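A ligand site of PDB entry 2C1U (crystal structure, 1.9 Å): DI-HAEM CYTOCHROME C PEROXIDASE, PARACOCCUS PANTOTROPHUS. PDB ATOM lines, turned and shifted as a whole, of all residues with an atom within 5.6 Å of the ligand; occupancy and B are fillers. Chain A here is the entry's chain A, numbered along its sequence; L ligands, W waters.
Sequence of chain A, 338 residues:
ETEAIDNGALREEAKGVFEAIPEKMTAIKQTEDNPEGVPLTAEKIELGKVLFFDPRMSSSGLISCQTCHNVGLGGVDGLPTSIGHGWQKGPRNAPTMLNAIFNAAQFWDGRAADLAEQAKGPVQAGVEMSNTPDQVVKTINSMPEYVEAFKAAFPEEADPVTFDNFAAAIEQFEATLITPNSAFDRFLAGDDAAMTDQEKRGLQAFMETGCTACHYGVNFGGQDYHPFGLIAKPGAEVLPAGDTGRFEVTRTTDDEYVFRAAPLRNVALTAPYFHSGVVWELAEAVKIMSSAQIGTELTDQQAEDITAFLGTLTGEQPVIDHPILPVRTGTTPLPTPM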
ATOM      1  N   PHE A  52     -15.145  29.866   7.675  1.00  0.00           N
ATOM      2  CA  PHE A  52     -15.650  28.922   8.665  1.00  0.00           C
ATOM      3  C   PHE A  52     -14.562  28.284   9.530  1.00  0.00           C
ATOM      4  O   PHE A  52     -14.775  28.028  10.710  1.00  0.00           O
ATOM      5  CB  PHE A  52     -16.341  27.807   7.908  1.00  0.00           C
ATOM      6  CG  PHE A  52     -17.169  26.906   8.766  1.00  0.00           C
ATOM      7  CD1 PHE A  52     -18.531  27.202   9.012  1.00  0.00           C
ATOM      8  CD2 PHE A  52     -16.617  25.738   9.301  1.00  0.00           C
ATOM      9  CE1 PHE A  52     -19.280  26.401   9.802  1.00  0.00           C
ATOM     10  CE2 PHE A  52     -17.408  24.861  10.104  1.00  0.00           C
ATOM     11  CZ  PHE A  52     -18.731  25.222  10.385  1.00  0.00           C
ATOM     12  N   ILE A  63     -10.732  30.393  18.271  1.00  0.00           N
ATOM     13  CA  ILE A  63     -12.107  29.910  18.085  1.00  0.00           C
ATOM     14  C   ILE A  63     -12.579  30.197  16.680  1.00  0.00           C
ATOM     15  O   ILE A  63     -12.613  31.350  16.291  1.00  0.00           O
ATOM     16  CB  ILE A  63     -13.074  30.597  19.065  1.00  0.00           C
ATOM     17  CG1 ILE A  63     -12.625  30.438  20.524  1.00  0.00           C
ATOM     18  CG2 ILE A  63     -14.461  29.987  18.913  1.00  0.00           C
ATOM     19  CD1 ILE A  63     -12.552  29.016  20.921  1.00  0.00           C
ATOM     20  N   SER A  64     -12.944  29.163  15.933  1.00  0.00           N
ATOM     21  CA  SER A  64     -13.489  29.387  14.580  1.00  0.00           C
ATOM     22  C   SER A  64     -14.942  28.863  14.622  1.00  0.00           C
ATOM     23  O   SER A  64     -15.346  28.251  15.647  1.00  0.00           O
ATOM     24  CB  SER A  64     -12.619  28.597  13.582  1.00  0.00           C
ATOM     25  OG  SER A  64     -12.789  27.199  13.812  1.00  0.00           O
ATOM     26  N   CYS A  65     -15.743  29.086  13.561  1.00  0.00           N
ATOM     27  CA  CYS A  65     -17.017  28.445  13.507  1.00  0.00           C
ATOM     28  C   CYS A  65     -16.890  26.925  13.684  1.00  0.00           C
ATOM     29  O   CYS A  65     -17.687  26.312  14.403  1.00  0.00           O
ATOM     30  CB  CYS A  65     -17.750  28.702  12.155  1.00  0.00           C
ATOM     31  SG  CYS A  65     -17.619  30.373  11.500  1.00  0.00           S
ATOM     32  N   THR A  67     -14.887  25.263  15.425  1.00  0.00           N
ATOM     33  CA  THR A  67     -14.788  24.860  16.848  1.00  0.00           C
ATOM     34  C   THR A  67     -16.127  24.378  17.447  1.00  0.00           C
ATOM     35  O   THR A  67     -16.200  23.309  18.054  1.00  0.00           O
ATOM     36  CB  THR A  67     -14.242  26.040  17.667  1.00  0.00           C
ATOM     37  OG1 THR A  67     -13.002  26.418  17.094  1.00  0.00           O
ATOM     38  CG2 THR A  67     -13.913  25.631  19.141  1.00  0.00           C
ATOM     39  N   CYS A  68     -17.182  25.154  17.275  1.00  0.00           N
ATOM     40  CA  CYS A  68     -18.473  24.857  17.934  1.00  0.00           C
ATOM     41  C   CYS A  68     -19.416  24.093  17.018  1.00  0.00           C
ATOM     42  O   CYS A  68     -20.344  23.480  17.489  1.00  0.00           O
ATOM     43  CB  CYS A  68     -19.170  26.145  18.379  1.00  0.00           C
ATOM     44  SG  CYS A  68     -18.203  27.096  19.649  1.00  0.00           S
ATOM     45  N   HIS A  69     -19.213  24.193  15.710  1.00  0.00           N
ATOM     46  CA  HIS A  69     -19.999  23.447  14.749  1.00  0.00           C
ATOM     47  C   HIS A  69     -19.125  22.472  13.931  1.00  0.00           C
ATOM     48  O   HIS A  69     -19.155  22.464  12.711  1.00  0.00           O
ATOM     49  CB  HIS A  69     -20.697  24.426  13.832  1.00  0.00           C
ATOM     50  CG  HIS A  69     -21.538  25.459  14.568  1.00  0.00           C
ATOM     51  ND1 HIS A  69     -22.771  25.168  15.091  1.00  0.00           N
ATOM     52  CD2 HIS A  69     -21.328  26.783  14.808  1.00  0.00           C
ATOM     53  CE1 HIS A  69     -23.318  26.267  15.593  1.00  0.00           C
ATOM     54  NE2 HIS A  69     -22.444  27.270  15.454  1.00  0.00           N
ATOM     55  N   ASP A  77     -20.230  20.680  18.692  1.00  0.00           N
ATOM     56  CA  ASP A  77     -18.956  20.481  19.423  1.00  0.00           C
ATOM     57  C   ASP A  77     -19.081  19.323  20.432  1.00  0.00           C
ATOM     58  O   ASP A  77     -18.088  18.903  21.028  1.00  0.00           O
ATOM     59  CB  ASP A  77     -18.495  21.785  20.114  1.00  0.00           C
ATOM     60  CG  ASP A  77     -19.513  22.348  21.118  1.00  0.00           C
ATOM     61  OD1 ASP A  77     -20.537  21.671  21.456  1.00  0.00           O
ATOM     62  OD2 ASP A  77     -19.389  23.523  21.612  1.00  0.00           O
ATOM     63  N   SER A  82     -22.339  26.621  25.036  1.00  0.00           N
ATOM     64  CA  SER A  82     -21.352  27.655  24.737  1.00  0.00           C
ATOM     65  C   SER A  82     -22.044  28.965  24.439  1.00  0.00           C
ATOM     66  O   SER A  82     -23.284  29.030  24.291  1.00  0.00           O
ATOM     67  CB  SER A  82     -20.464  27.244  23.550  1.00  0.00           C
ATOM     68  OG  SER A  82     -21.240  26.665  22.493  1.00  0.00           O
ATOM     69  N   ILE A  83     -21.217  30.008  24.371  1.00  0.00           N
ATOM     70  CA  ILE A  83     -21.692  31.298  23.890  1.00  0.00           C
ATOM     71  C   ILE A  83     -20.910  31.677  22.640  1.00  0.00           C
ATOM     72  O   ILE A  83     -19.716  32.000  22.694  1.00  0.00           O
ATOM     73  CB  ILE A  83     -21.575  32.392  24.967  1.00  0.00           C
ATOM     74  CG1 ILE A  83     -22.472  32.038  26.154  1.00  0.00           C
ATOM     75  CG2 ILE A  83     -21.949  33.759  24.328  1.00  0.00           C
ATOM     76  CD1 ILE A  83     -22.426  33.030  27.322  1.00  0.00           C
ATOM     77  N   GLY A  84     -21.597  31.640  21.516  1.00  0.00           N
ATOM     78  CA  GLY A  84     -20.935  31.964  20.271  1.00  0.00           C
ATOM     79  C   GLY A  84     -21.530  33.127  19.532  1.00  0.00           C
ATOM     80  O   GLY A  84     -20.897  33.616  18.620  1.00  0.00           O
ATOM     81  N   HIS A  85     -22.736  33.551  19.903  1.00  0.00           N
ATOM     82  CA  HIS A  85     -23.439  34.604  19.150  1.00  0.00           C
ATOM     83  C   HIS A  85     -24.012  35.705  20.045  1.00  0.00           C
ATOM     84  O   HIS A  85     -24.570  35.410  21.099  1.00  0.00           O
ATOM     85  CB  HIS A  85     -24.530  33.997  18.255  1.00  0.00           C
ATOM     86  CG  HIS A  85     -23.989  32.942  17.351  1.00  0.00           C
ATOM     87  ND1 HIS A  85     -23.436  33.229  16.126  1.00  0.00           N
ATOM     88  CD2 HIS A  85     -23.863  31.609  17.522  1.00  0.00           C
ATOM     89  CE1 HIS A  85     -23.022  32.104  15.562  1.00  0.00           C
ATOM     90  NE2 HIS A  85     -23.285  31.108  16.382  1.00  0.00           N
ATOM     91  N   GLN A  88     -27.521  35.569  21.973  1.00  0.00           N
ATOM     92  CA  GLN A  88     -27.754  34.669  23.143  1.00  0.00           C
ATOM     93  C   GLN A  88     -27.996  35.417  24.471  1.00  0.00           C
ATOM     94  O   GLN A  88     -27.265  36.343  24.773  1.00  0.00           O
ATOM     95  CB  GLN A  88     -26.589  33.686  23.317  1.00  0.00           C
ATOM     96  CG  GLN A  88     -26.450  32.659  22.192  1.00  0.00           C
ATOM     97  CD  GLN A  88     -25.315  31.699  22.433  1.00  0.00           C
ATOM     98  OE1 GLN A  88     -24.325  31.664  21.655  1.00  0.00           O
ATOM     99  NE2 GLN A  88     -25.423  30.921  23.502  1.00  0.00           N
ATOM    100  N   ARG A  92     -25.947  28.165  25.545  1.00  0.00           N
ATOM    101  CA  ARG A  92     -26.823  27.191  24.905  1.00  0.00           C
ATOM    102  C   ARG A  92     -25.989  26.133  24.235  1.00  0.00           C
ATOM    103  O   ARG A  92     -24.824  26.350  23.867  1.00  0.00           O
ATOM    104  CB  ARG A  92     -27.688  27.833  23.814  1.00  0.00           C
ATOM    105  CG  ARG A  92     -28.685  28.847  24.322  1.00  0.00           C
ATOM    106  CD  ARG A  92     -29.801  28.213  25.092  1.00  0.00           C
ATOM    107  NE  ARG A  92     -30.857  29.142  25.509  1.00  0.00           N
ATOM    108  CZ  ARG A  92     -30.849  29.819  26.630  1.00  0.00           C
ATOM    109  NH1 ARG A  92     -29.801  29.755  27.473  1.00  0.00           N
ATOM    110  NH2 ARG A  92     -31.885  30.588  26.920  1.00  0.00           N
ATOM    111  N   ASN A  93     -26.639  24.984  24.039  1.00  0.00           N
ATOM    112  CA  ASN A  93     -26.080  23.892  23.282  1.00  0.00           C
ATOM    113  C   ASN A  93     -25.992  24.308  21.816  1.00  0.00           C
ATOM    114  O   ASN A  93     -26.997  24.775  21.221  1.00  0.00           O
ATOM    115  CB  ASN A  93     -27.008  22.675  23.419  1.00  0.00           C
ATOM    116  CG  ASN A  93     -26.416  21.448  22.819  1.00  0.00           C
ATOM    117  OD1 ASN A  93     -26.891  20.936  21.834  1.00  0.00           O
ATOM    118  ND2 ASN A  93     -25.314  21.012  23.398  1.00  0.00           N
ATOM    119  N   ALA A  94     -24.819  24.128  21.207  1.00  0.00           N
ATOM    120  CA  ALA A  94     -24.662  24.480  19.800  1.00  0.00           C
ATOM    121  C   ALA A  94     -25.471  23.545  18.902  1.00  0.00           C
ATOM    122  O   ALA A  94     -25.313  22.328  18.998  1.00  0.00           O
ATOM    123  CB  ALA A  94     -23.207  24.421  19.426  1.00  0.00           C
ATOM    124  N   PRO A  95     -26.382  24.099  18.091  1.00  0.00           N
ATOM    125  CA  PRO A  95     -27.125  23.306  17.116  1.00  0.00           C
ATOM    126  C   PRO A  95     -26.205  22.915  15.962  1.00  0.00           C
ATOM    127  O   PRO A  95     -25.213  23.599  15.676  1.00  0.00           O
ATOM    128  CB  PRO A  95     -28.230  24.259  16.626  1.00  0.00           C
ATOM    129  CG  PRO A  95     -27.671  25.592  16.776  1.00  0.00           C
ATOM    130  CD  PRO A  95     -26.774  25.518  18.032  1.00  0.00           C
ATOM    131  N   THR A  96     -26.522  21.815  15.287  1.00  0.00           N
ATOM    132  CA  THR A  96     -25.755  21.421  14.139  1.00  0.00           C
ATOM    133  C   THR A  96     -25.863  22.407  12.951  1.00  0.00           C
ATOM    134  O   THR A  96     -26.965  22.904  12.608  1.00  0.00           O
ATOM    135  CB  THR A  96     -26.157  19.978  13.706  1.00  0.00           C
ATOM    136  OG1 THR A  96     -25.290  19.541  12.650  1.00  0.00           O
ATOM    137  CG2 THR A  96     -27.588  19.924  13.068  1.00  0.00           C
ATOM    138  N   MET A  97     -24.734  22.639  12.304  1.00  0.00           N
ATOM    139  CA  MET A  97     -24.712  23.325  10.993  1.00  0.00           C
ATOM    140  C   MET A  97     -25.271  22.437   9.903  1.00  0.00           C
ATOM    141  O   MET A  97     -25.682  22.951   8.855  1.00  0.00           O
ATOM    142  CB  MET A  97     -23.282  23.666  10.585  1.00  0.00           C
ATOM    143  CG  MET A  97     -23.188  24.658   9.443  1.00  0.00           C
ATOM    144  SD  MET A  97     -23.579  26.325  10.062  1.00  0.00           S
ATOM    145  CE  MET A  97     -22.862  26.289  11.655  1.00  0.00           C
ATOM    146  N   ALA A 100     -28.726  23.130   8.421  1.00  0.00           N
ATOM    147  CA  ALA A 100     -29.254  24.379   9.043  1.00  0.00           C
ATOM    148  C   ALA A 100     -29.851  25.328   8.026  1.00  0.00           C
ATOM    149  O   ALA A 100     -30.764  26.101   8.300  1.00  0.00           O
ATOM    150  CB  ALA A 100     -28.175  25.097   9.910  1.00  0.00           C
ATOM    151  N   ASN A 103     -33.774  25.518   8.038  1.00  0.00           N
ATOM    152  CA  ASN A 103     -34.550  25.918   9.195  1.00  0.00           C
ATOM    153  C   ASN A 103     -35.071  27.333   9.075  1.00  0.00           C
ATOM    154  O   ASN A 103     -34.263  28.273   9.064  1.00  0.00           O
ATOM    155  CB  ASN A 103     -33.688  25.824  10.493  1.00  0.00           C
ATOM    156  CG  ASN A 103     -33.147  24.449  10.758  1.00  0.00           C
ATOM    157  OD1 ASN A 103     -33.777  23.461  10.458  1.00  0.00           O
ATOM    158  ND2 ASN A 103     -31.937  24.384  11.366  1.00  0.00           N
ATOM    159  N   ALA A 105     -36.883  28.755  11.438  1.00  0.00           N
ATOM    160  CA  ALA A 105     -36.705  29.286  12.795  1.00  0.00           C
ATOM    161  C   ALA A 105     -35.217  29.167  13.092  1.00  0.00           C
ATOM    162  O   ALA A 105     -34.651  28.093  12.950  1.00  0.00           O
ATOM    163  CB  ALA A 105     -37.501  28.425  13.778  1.00  0.00           C
ATOM    164  N   GLN A 106     -34.583  30.275  13.514  1.00  0.00           N
ATOM    165  CA  GLN A 106     -33.104  30.338  13.522  1.00  0.00           C
ATOM    166  C   GLN A 106     -32.467  30.321  14.902  1.00  0.00           C
ATOM    167  O   GLN A 106     -31.218  30.230  14.996  1.00  0.00           O
ATOM    168  CB  GLN A 106     -32.610  31.598  12.788  1.00  0.00           C
ATOM    169  CG  GLN A 106     -33.369  31.889  11.476  1.00  0.00           C
ATOM    170  CD  GLN A 106     -33.147  33.281  10.953  1.00  0.00           C
ATOM    171  OE1 GLN A 106     -33.665  34.254  11.510  1.00  0.00           O
ATOM    172  NE2 GLN A 106     -32.405  33.390   9.878  1.00  0.00           N
ATOM    173  N   PHE A 107     -33.291  30.389  15.944  1.00  0.00           N
ATOM    174  CA  PHE A 107     -32.783  30.514  17.319  1.00  0.00           C
ATOM    175  C   PHE A 107     -33.357  29.420  18.168  1.00  0.00           C
ATOM    176  O   PHE A 107     -34.422  28.877  17.847  1.00  0.00           O
ATOM    177  CB  PHE A 107     -33.143  31.911  17.892  1.00  0.00           C
ATOM    178  CG  PHE A 107     -32.447  33.051  17.194  1.00  0.00           C
ATOM    179  CD1 PHE A 107     -31.091  33.291  17.423  1.00  0.00           C
ATOM    180  CD2 PHE A 107     -33.122  33.853  16.288  1.00  0.00           C
ATOM    181  CE1 PHE A 107     -30.422  34.333  16.768  1.00  0.00           C
ATOM    182  CE2 PHE A 107     -32.473  34.899  15.633  1.00  0.00           C
ATOM    183  CZ  PHE A 107     -31.127  35.144  15.871  1.00  0.00           C
ATOM    184  N   TRP A 108     -32.682  29.120  19.278  1.00  0.00           N
ATOM    185  CA  TRP A 108     -33.169  28.160  20.263  1.00  0.00           C
ATOM    186  C   TRP A 108     -34.418  28.652  20.943  1.00  0.00           C
ATOM    187  O   TRP A 108     -35.336  27.894  21.118  1.00  0.00           O
ATOM    188  CB  TRP A 108     -32.137  27.872  21.369  1.00  0.00           C
ATOM    189  CG  TRP A 108     -31.325  26.617  21.191  1.00  0.00           C
ATOM    190  CD1 TRP A 108     -29.974  26.524  20.998  1.00  0.00           C
ATOM    191  CD2 TRP A 108     -31.814  25.260  21.214  1.00  0.00           C
ATOM    192  NE1 TRP A 108     -29.582  25.198  20.918  1.00  0.00           N
ATOM    193  CE2 TRP A 108     -30.695  24.409  21.046  1.00  0.00           C
ATOM    194  CE3 TRP A 108     -33.088  24.689  21.392  1.00  0.00           C
ATOM    195  CZ2 TRP A 108     -30.813  23.016  21.009  1.00  0.00           C
ATOM    196  CZ3 TRP A 108     -33.197  23.285  21.360  1.00  0.00           C
ATOM    197  CH2 TRP A 108     -32.072  22.474  21.185  1.00  0.00           C
ATOM    198  N   ASP A 109     -34.448  29.923  21.366  1.00  0.00           N
ATOM    199  CA  ASP A 109     -35.534  30.396  22.215  1.00  0.00           C
ATOM    200  C   ASP A 109     -35.569  31.924  22.295  1.00  0.00           C
ATOM    201  O   ASP A 109     -34.595  32.605  21.945  1.00  0.00           O
ATOM    202  CB  ASP A 109     -35.389  29.837  23.629  1.00  0.00           C
ATOM    203  CG  ASP A 109     -34.073  30.265  24.290  1.00  0.00           C
ATOM    204  OD1 ASP A 109     -32.986  29.833  23.828  1.00  0.00           O
ATOM    205  OD2 ASP A 109     -34.021  31.048  25.266  1.00  0.00           O
ATOM    206  N   PRO A 122     -28.392  33.759  13.609  1.00  0.00           N
ATOM    207  CA  PRO A 122     -27.349  33.903  14.644  1.00  0.00           C
ATOM    208  C   PRO A 122     -26.062  34.617  14.194  1.00  0.00           C
ATOM    209  O   PRO A 122     -25.505  35.398  14.971  1.00  0.00           O
ATOM    210  CB  PRO A 122     -27.060  32.443  15.041  1.00  0.00           C
ATOM    211  CG  PRO A 122     -28.316  31.724  14.748  1.00  0.00           C
ATOM    212  CD  PRO A 122     -28.800  32.349  13.446  1.00  0.00           C
ATOM    213  N   VAL A 123     -25.610  34.385  12.961  1.00  0.00           N
ATOM    214  CA  VAL A 123     -24.332  34.970  12.493  1.00  0.00           C
ATOM    215  C   VAL A 123     -24.361  36.511  12.479  1.00  0.00           C
ATOM    216  O   VAL A 123     -23.362  37.154  12.824  1.00  0.00           O
ATOM    217  CB  VAL A 123     -23.919  34.392  11.118  1.00  0.00           C
ATOM    218  CG1 VAL A 123     -22.637  35.052  10.594  1.00  0.00           C
ATOM    219  CG2 VAL A 123     -23.746  32.888  11.221  1.00  0.00           C
ATOM    220  N   PHE A 166     -18.938  38.529   4.252  1.00  0.00           N
ATOM    221  CA  PHE A 166     -18.463  37.477   5.142  1.00  0.00           C
ATOM    222  C   PHE A 166     -19.665  36.550   5.421  1.00  0.00           C
ATOM    223  O   PHE A 166     -19.559  35.326   5.281  1.00  0.00           O
ATOM    224  CB  PHE A 166     -17.904  38.153   6.403  1.00  0.00           C
ATOM    225  CG  PHE A 166     -17.604  37.228   7.581  1.00  0.00           C
ATOM    226  CD1 PHE A 166     -18.566  36.990   8.576  1.00  0.00           C
ATOM    227  CD2 PHE A 166     -16.345  36.714   7.774  1.00  0.00           C
ATOM    228  CE1 PHE A 166     -18.267  36.179   9.736  1.00  0.00           C
ATOM    229  CE2 PHE A 166     -16.036  35.911   8.930  1.00  0.00           C
ATOM    230  CZ  PHE A 166     -17.012  35.632   9.879  1.00  0.00           C
ATOM    231  N   ILE A 170     -20.182  32.498   3.946  1.00  0.00           N
ATOM    232  CA  ILE A 170     -20.429  31.385   4.883  1.00  0.00           C
ATOM    233  C   ILE A 170     -21.773  30.692   4.613  1.00  0.00           C
ATOM    234  O   ILE A 170     -21.826  29.463   4.622  1.00  0.00           O
ATOM    235  CB  ILE A 170     -20.269  31.832   6.343  1.00  0.00           C
ATOM    236  CG1 ILE A 170     -18.804  32.194   6.592  1.00  0.00           C
ATOM    237  CG2 ILE A 170     -20.516  30.643   7.259  1.00  0.00           C
ATOM    238  CD1 ILE A 170     -18.568  32.889   7.918  1.00  0.00           C
ATOM    239  N   GLU A 174     -22.474  26.974   3.936  1.00  0.00           N
ATOM    240  CA  GLU A 174     -23.491  26.273   4.745  1.00  0.00           C
ATOM    241  C   GLU A 174     -24.440  25.429   3.897  1.00  0.00           C
ATOM    242  O   GLU A 174     -24.803  24.333   4.304  1.00  0.00           O
ATOM    243  CB  GLU A 174     -24.261  27.236   5.674  1.00  0.00           C
ATOM    244  CG  GLU A 174     -25.655  26.746   6.136  1.00  0.00           C
ATOM    245  CD  GLU A 174     -26.509  27.855   6.763  1.00  0.00           C
ATOM    246  OE1 GLU A 174     -26.511  28.991   6.250  1.00  0.00           O
ATOM    247  OE2 GLU A 174     -27.170  27.605   7.778  1.00  0.00           O
ATOM    248  N   ARG A 260     -37.637  26.683  19.977  1.00  0.00           N
ATOM    249  CA  ARG A 260     -37.748  26.079  18.683  1.00  0.00           C
ATOM    250  C   ARG A 260     -37.833  24.542  18.786  1.00  0.00           C
ATOM    251  O   ARG A 260     -37.037  23.935  19.481  1.00  0.00           O
ATOM    252  CB  ARG A 260     -36.483  26.503  17.925  1.00  0.00           C
ATOM    253  CG  ARG A 260     -36.244  25.700  16.720  1.00  0.00           C
ATOM    254  CD  ARG A 260     -34.803  25.207  16.735  1.00  0.00           C
ATOM    255  NE  ARG A 260     -34.238  25.849  15.616  1.00  0.00           N
ATOM    256  CZ  ARG A 260     -33.049  25.674  15.125  1.00  0.00           C
ATOM    257  NH1 ARG A 260     -32.139  24.852  15.682  1.00  0.00           N
ATOM    258  NH2 ARG A 260     -32.793  26.355  14.018  1.00  0.00           N
ATOM    259  N   PRO A 263     -34.676  20.532  15.191  1.00  0.00           N
ATOM    260  CA  PRO A 263     -34.650  19.719  13.953  1.00  0.00           C
ATOM    261  C   PRO A 263     -33.919  18.399  14.243  1.00  0.00           C
ATOM    262  O   PRO A 263     -32.753  18.402  14.713  1.00  0.00           O
ATOM    263  CB  PRO A 263     -33.897  20.617  12.933  1.00  0.00           C
ATOM    264  CG  PRO A 263     -32.947  21.489  13.845  1.00  0.00           C
ATOM    265  CD  PRO A 263     -33.788  21.707  15.117  1.00  0.00           C
HETATM  266 FE1  LIG L   1     -22.874  29.208  15.844  1.00  0.00          FE
HETATM  267  C1  LIG L   1     -26.238  28.833  16.353  1.00  0.00           C
HETATM  268  C2  LIG L   1     -23.360  29.472  12.547  1.00  0.00           C
HETATM  269  C3  LIG L   1     -19.607  30.202  15.392  1.00  0.00           C
HETATM  270  C4  LIG L   1     -22.146  28.405  19.078  1.00  0.00           C
HETATM  271  N1  LIG L   1     -24.538  29.187  14.641  1.00  0.00           N
HETATM  272  C5  LIG L   1     -25.826  28.902  15.032  1.00  0.00           C
HETATM  273  C6  LIG L   1     -26.633  28.725  13.820  1.00  0.00           C
HETATM  274  C7  LIG L   1     -25.808  28.915  12.761  1.00  0.00           C
HETATM  275  C8  LIG L   1     -24.478  29.203  13.287  1.00  0.00           C
HETATM  276  C9  LIG L   1     -26.134  28.874  11.224  1.00  0.00           C
HETATM  277  C10 LIG L   1     -28.154  28.388  13.780  1.00  0.00           C
HETATM  278  C11 LIG L   1     -28.332  26.944  13.308  1.00  0.00           C
HETATM  279  C12 LIG L   1     -29.768  26.554  12.984  1.00  0.00           C
HETATM  280  O1  LIG L   1     -30.190  25.483  13.447  1.00  0.00           O
HETATM  281  O2  LIG L   1     -30.489  27.238  12.241  1.00  0.00           O
HETATM  282  N2  LIG L   1     -21.667  29.753  14.291  1.00  0.00           N
HETATM  283  C13 LIG L   1     -22.113  29.854  13.000  1.00  0.00           C
HETATM  284  C14 LIG L   1     -21.101  30.532  12.213  1.00  0.00           C
HETATM  285  C15 LIG L   1     -20.020  30.707  12.959  1.00  0.00           C
HETATM  286  C16 LIG L   1     -20.391  30.264  14.303  1.00  0.00           C
HETATM  287  C17 LIG L   1     -21.310  30.717  10.682  1.00  0.00           C
HETATM  288  C18 LIG L   1     -18.674  31.359  12.569  1.00  0.00           C
HETATM  289  C19 LIG L   1     -18.898  32.862  12.217  1.00  0.00           C
HETATM  290  N3  LIG L   1     -21.189  29.278  16.992  1.00  0.00           N
HETATM  291  C20 LIG L   1     -19.923  29.680  16.605  1.00  0.00           C
HETATM  292  C21 LIG L   1     -19.086  29.781  17.785  1.00  0.00           C
HETATM  293  C22 LIG L   1     -19.744  29.093  18.764  1.00  0.00           C
HETATM  294  C23 LIG L   1     -21.116  28.880  18.315  1.00  0.00           C
HETATM  295  C24 LIG L   1     -17.540  29.921  17.692  1.00  0.00           C
HETATM  296  C25 LIG L   1     -19.253  28.667  20.164  1.00  0.00           C
HETATM  297  C26 LIG L   1     -18.319  29.601  20.961  1.00  0.00           C
HETATM  298  N4  LIG L   1     -23.999  28.672  17.425  1.00  0.00           N
HETATM  299  C27 LIG L   1     -23.467  28.476  18.711  1.00  0.00           C
HETATM  300  C28 LIG L   1     -24.545  28.381  19.636  1.00  0.00           C
HETATM  301  C29 LIG L   1     -25.834  28.532  18.816  1.00  0.00           C
HETATM  302  C30 LIG L   1     -25.401  28.721  17.452  1.00  0.00           C
HETATM  303  C31 LIG L   1     -24.440  28.177  21.156  1.00  0.00           C
HETATM  304  C32 LIG L   1     -27.276  28.535  19.368  1.00  0.00           C
HETATM  305  C33 LIG L   1     -27.664  30.017  19.478  1.00  0.00           C
HETATM  306  C34 LIG L   1     -29.094  30.188  19.912  1.00  0.00           C
HETATM  307  O3  LIG L   1     -29.259  30.555  21.088  1.00  0.00           O
HETATM  308  O4  LIG L   1     -30.045  29.918  19.105  1.00  0.00           O
HETATM  309  O   HOH W   1     -30.095  28.493  16.893  1.00  0.00           O
HETATM  310  O   HOH W   2     -29.665  22.998  13.285  1.00  0.00           O
HETATM  311  O   HOH W   3     -31.331  31.546  22.259  1.00  0.00           O
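FE1 of the ligand is bound by NE2 of His 85 (2.0 Å). C25 of the ligand is covalently linked to SG of Cys 68 (2.0 Å). The backbone NH (N) of Trp 108 lies within hydrogen-bond range of an oxygen (O4) of the ligand. An iron atom (FE1) of the ligand is bound by a ring nitrogen (NE2) of His 69, at 2.0 Å. An oxygen (O1) of the ligand lies within salt-bridge range of the guanidinium group of Arg 260, 2.8 Å away. O1 of the ligand sits at hydrogen-bond distance from ND2 of Asn 103. A carbon (C18) of the ligand is bonded to the side-chain sulfur of Cys 65 (1.8 Å).
The backbone carbonyl oxygen (O) of Asn 93 is in hydrogen-bond range of the indole nitrogen (NE1) of Trp 108 (2.6 Å). NH2 of Arg 260 lies within hydrogen-bond range of O of Ala 105 (2.8 Å). The guanidinium group (NH2) of Arg 92 lies within salt-bridge range of the side-chain carboxylate (OD2) of Asp 109 (2.7 Å). The backbone carbonyl oxygen (O) of Arg 92 is in hydrogen-bond range of the backbone NH (N) of Ser 82 (2.8 Å). The guanidinium group (NH2) of Arg 260 sits close to the side-chain amide nitrogen (ND2) of Asn 103 (3.4 Å). O of Pro 122 lies within hydrogen-bond range of ND1 of His 85 (3.2 Å). The backbone NH (N) of Gly 84 is in hydrogen-bond range of the side-chain amide oxygen (OE1) of Gln 88 (2.7 Å). The side-chain amide oxygen (OE1) of Gln 88 is in hydrogen-bond range of the backbone NH (N) of His 85.
Ile 63 touches the ligand. Ser 64 touches the ligand. Ser 82 touches the ligand (O to C31, 3.4 Å). O of Ile 83 touches C26 of the ligand (3.3 Å). CA of Gly 84 touches C22 of the ligand, at 3.5 Å. Gln 88 touches the ligand. Arg 92 touches the ligand. Ala 94 touches the ligand. Pro 95 touches the ligand. CE of Met 97 touches C2 of the ligand (3.3 Å). Ala 100 touches the ligand. Gln 106 touches the ligand. CA of Phe 107 touches O4 of the ligand (3.3 Å). CG of Pro 122 touches C10 of the ligand (3.5 Å). CG2 of Val 123 touches C17 of the ligand (3.3 Å). Ile 170 touches the ligand. Glu 174 touches the ligand (OE2 to C9, 3.8 Å). Of the 33 residues printed, 24 come within 4 Å of the ligand. Along chain A the residues within 4 Å of the ligand span positions 63 to 260.
Water W2 lies within hydrogen-bond range of an oxygen (O1) of the ligand (2.5 Å), the backbone carbonyl oxygen of Thr 96 (2.8 Å) and the side-chain amide nitrogen of Asn 103 (3.3 Å). Water W3 bridges an oxygen (O3) of the ligand (2.6 Å) and the side-chain carboxylate of Asp 109 (2.9 Å). Water W1 lies within hydrogen-bond range of O4 of the ligand (2.6 Å) and O of Gln 106 (2.8 Å).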
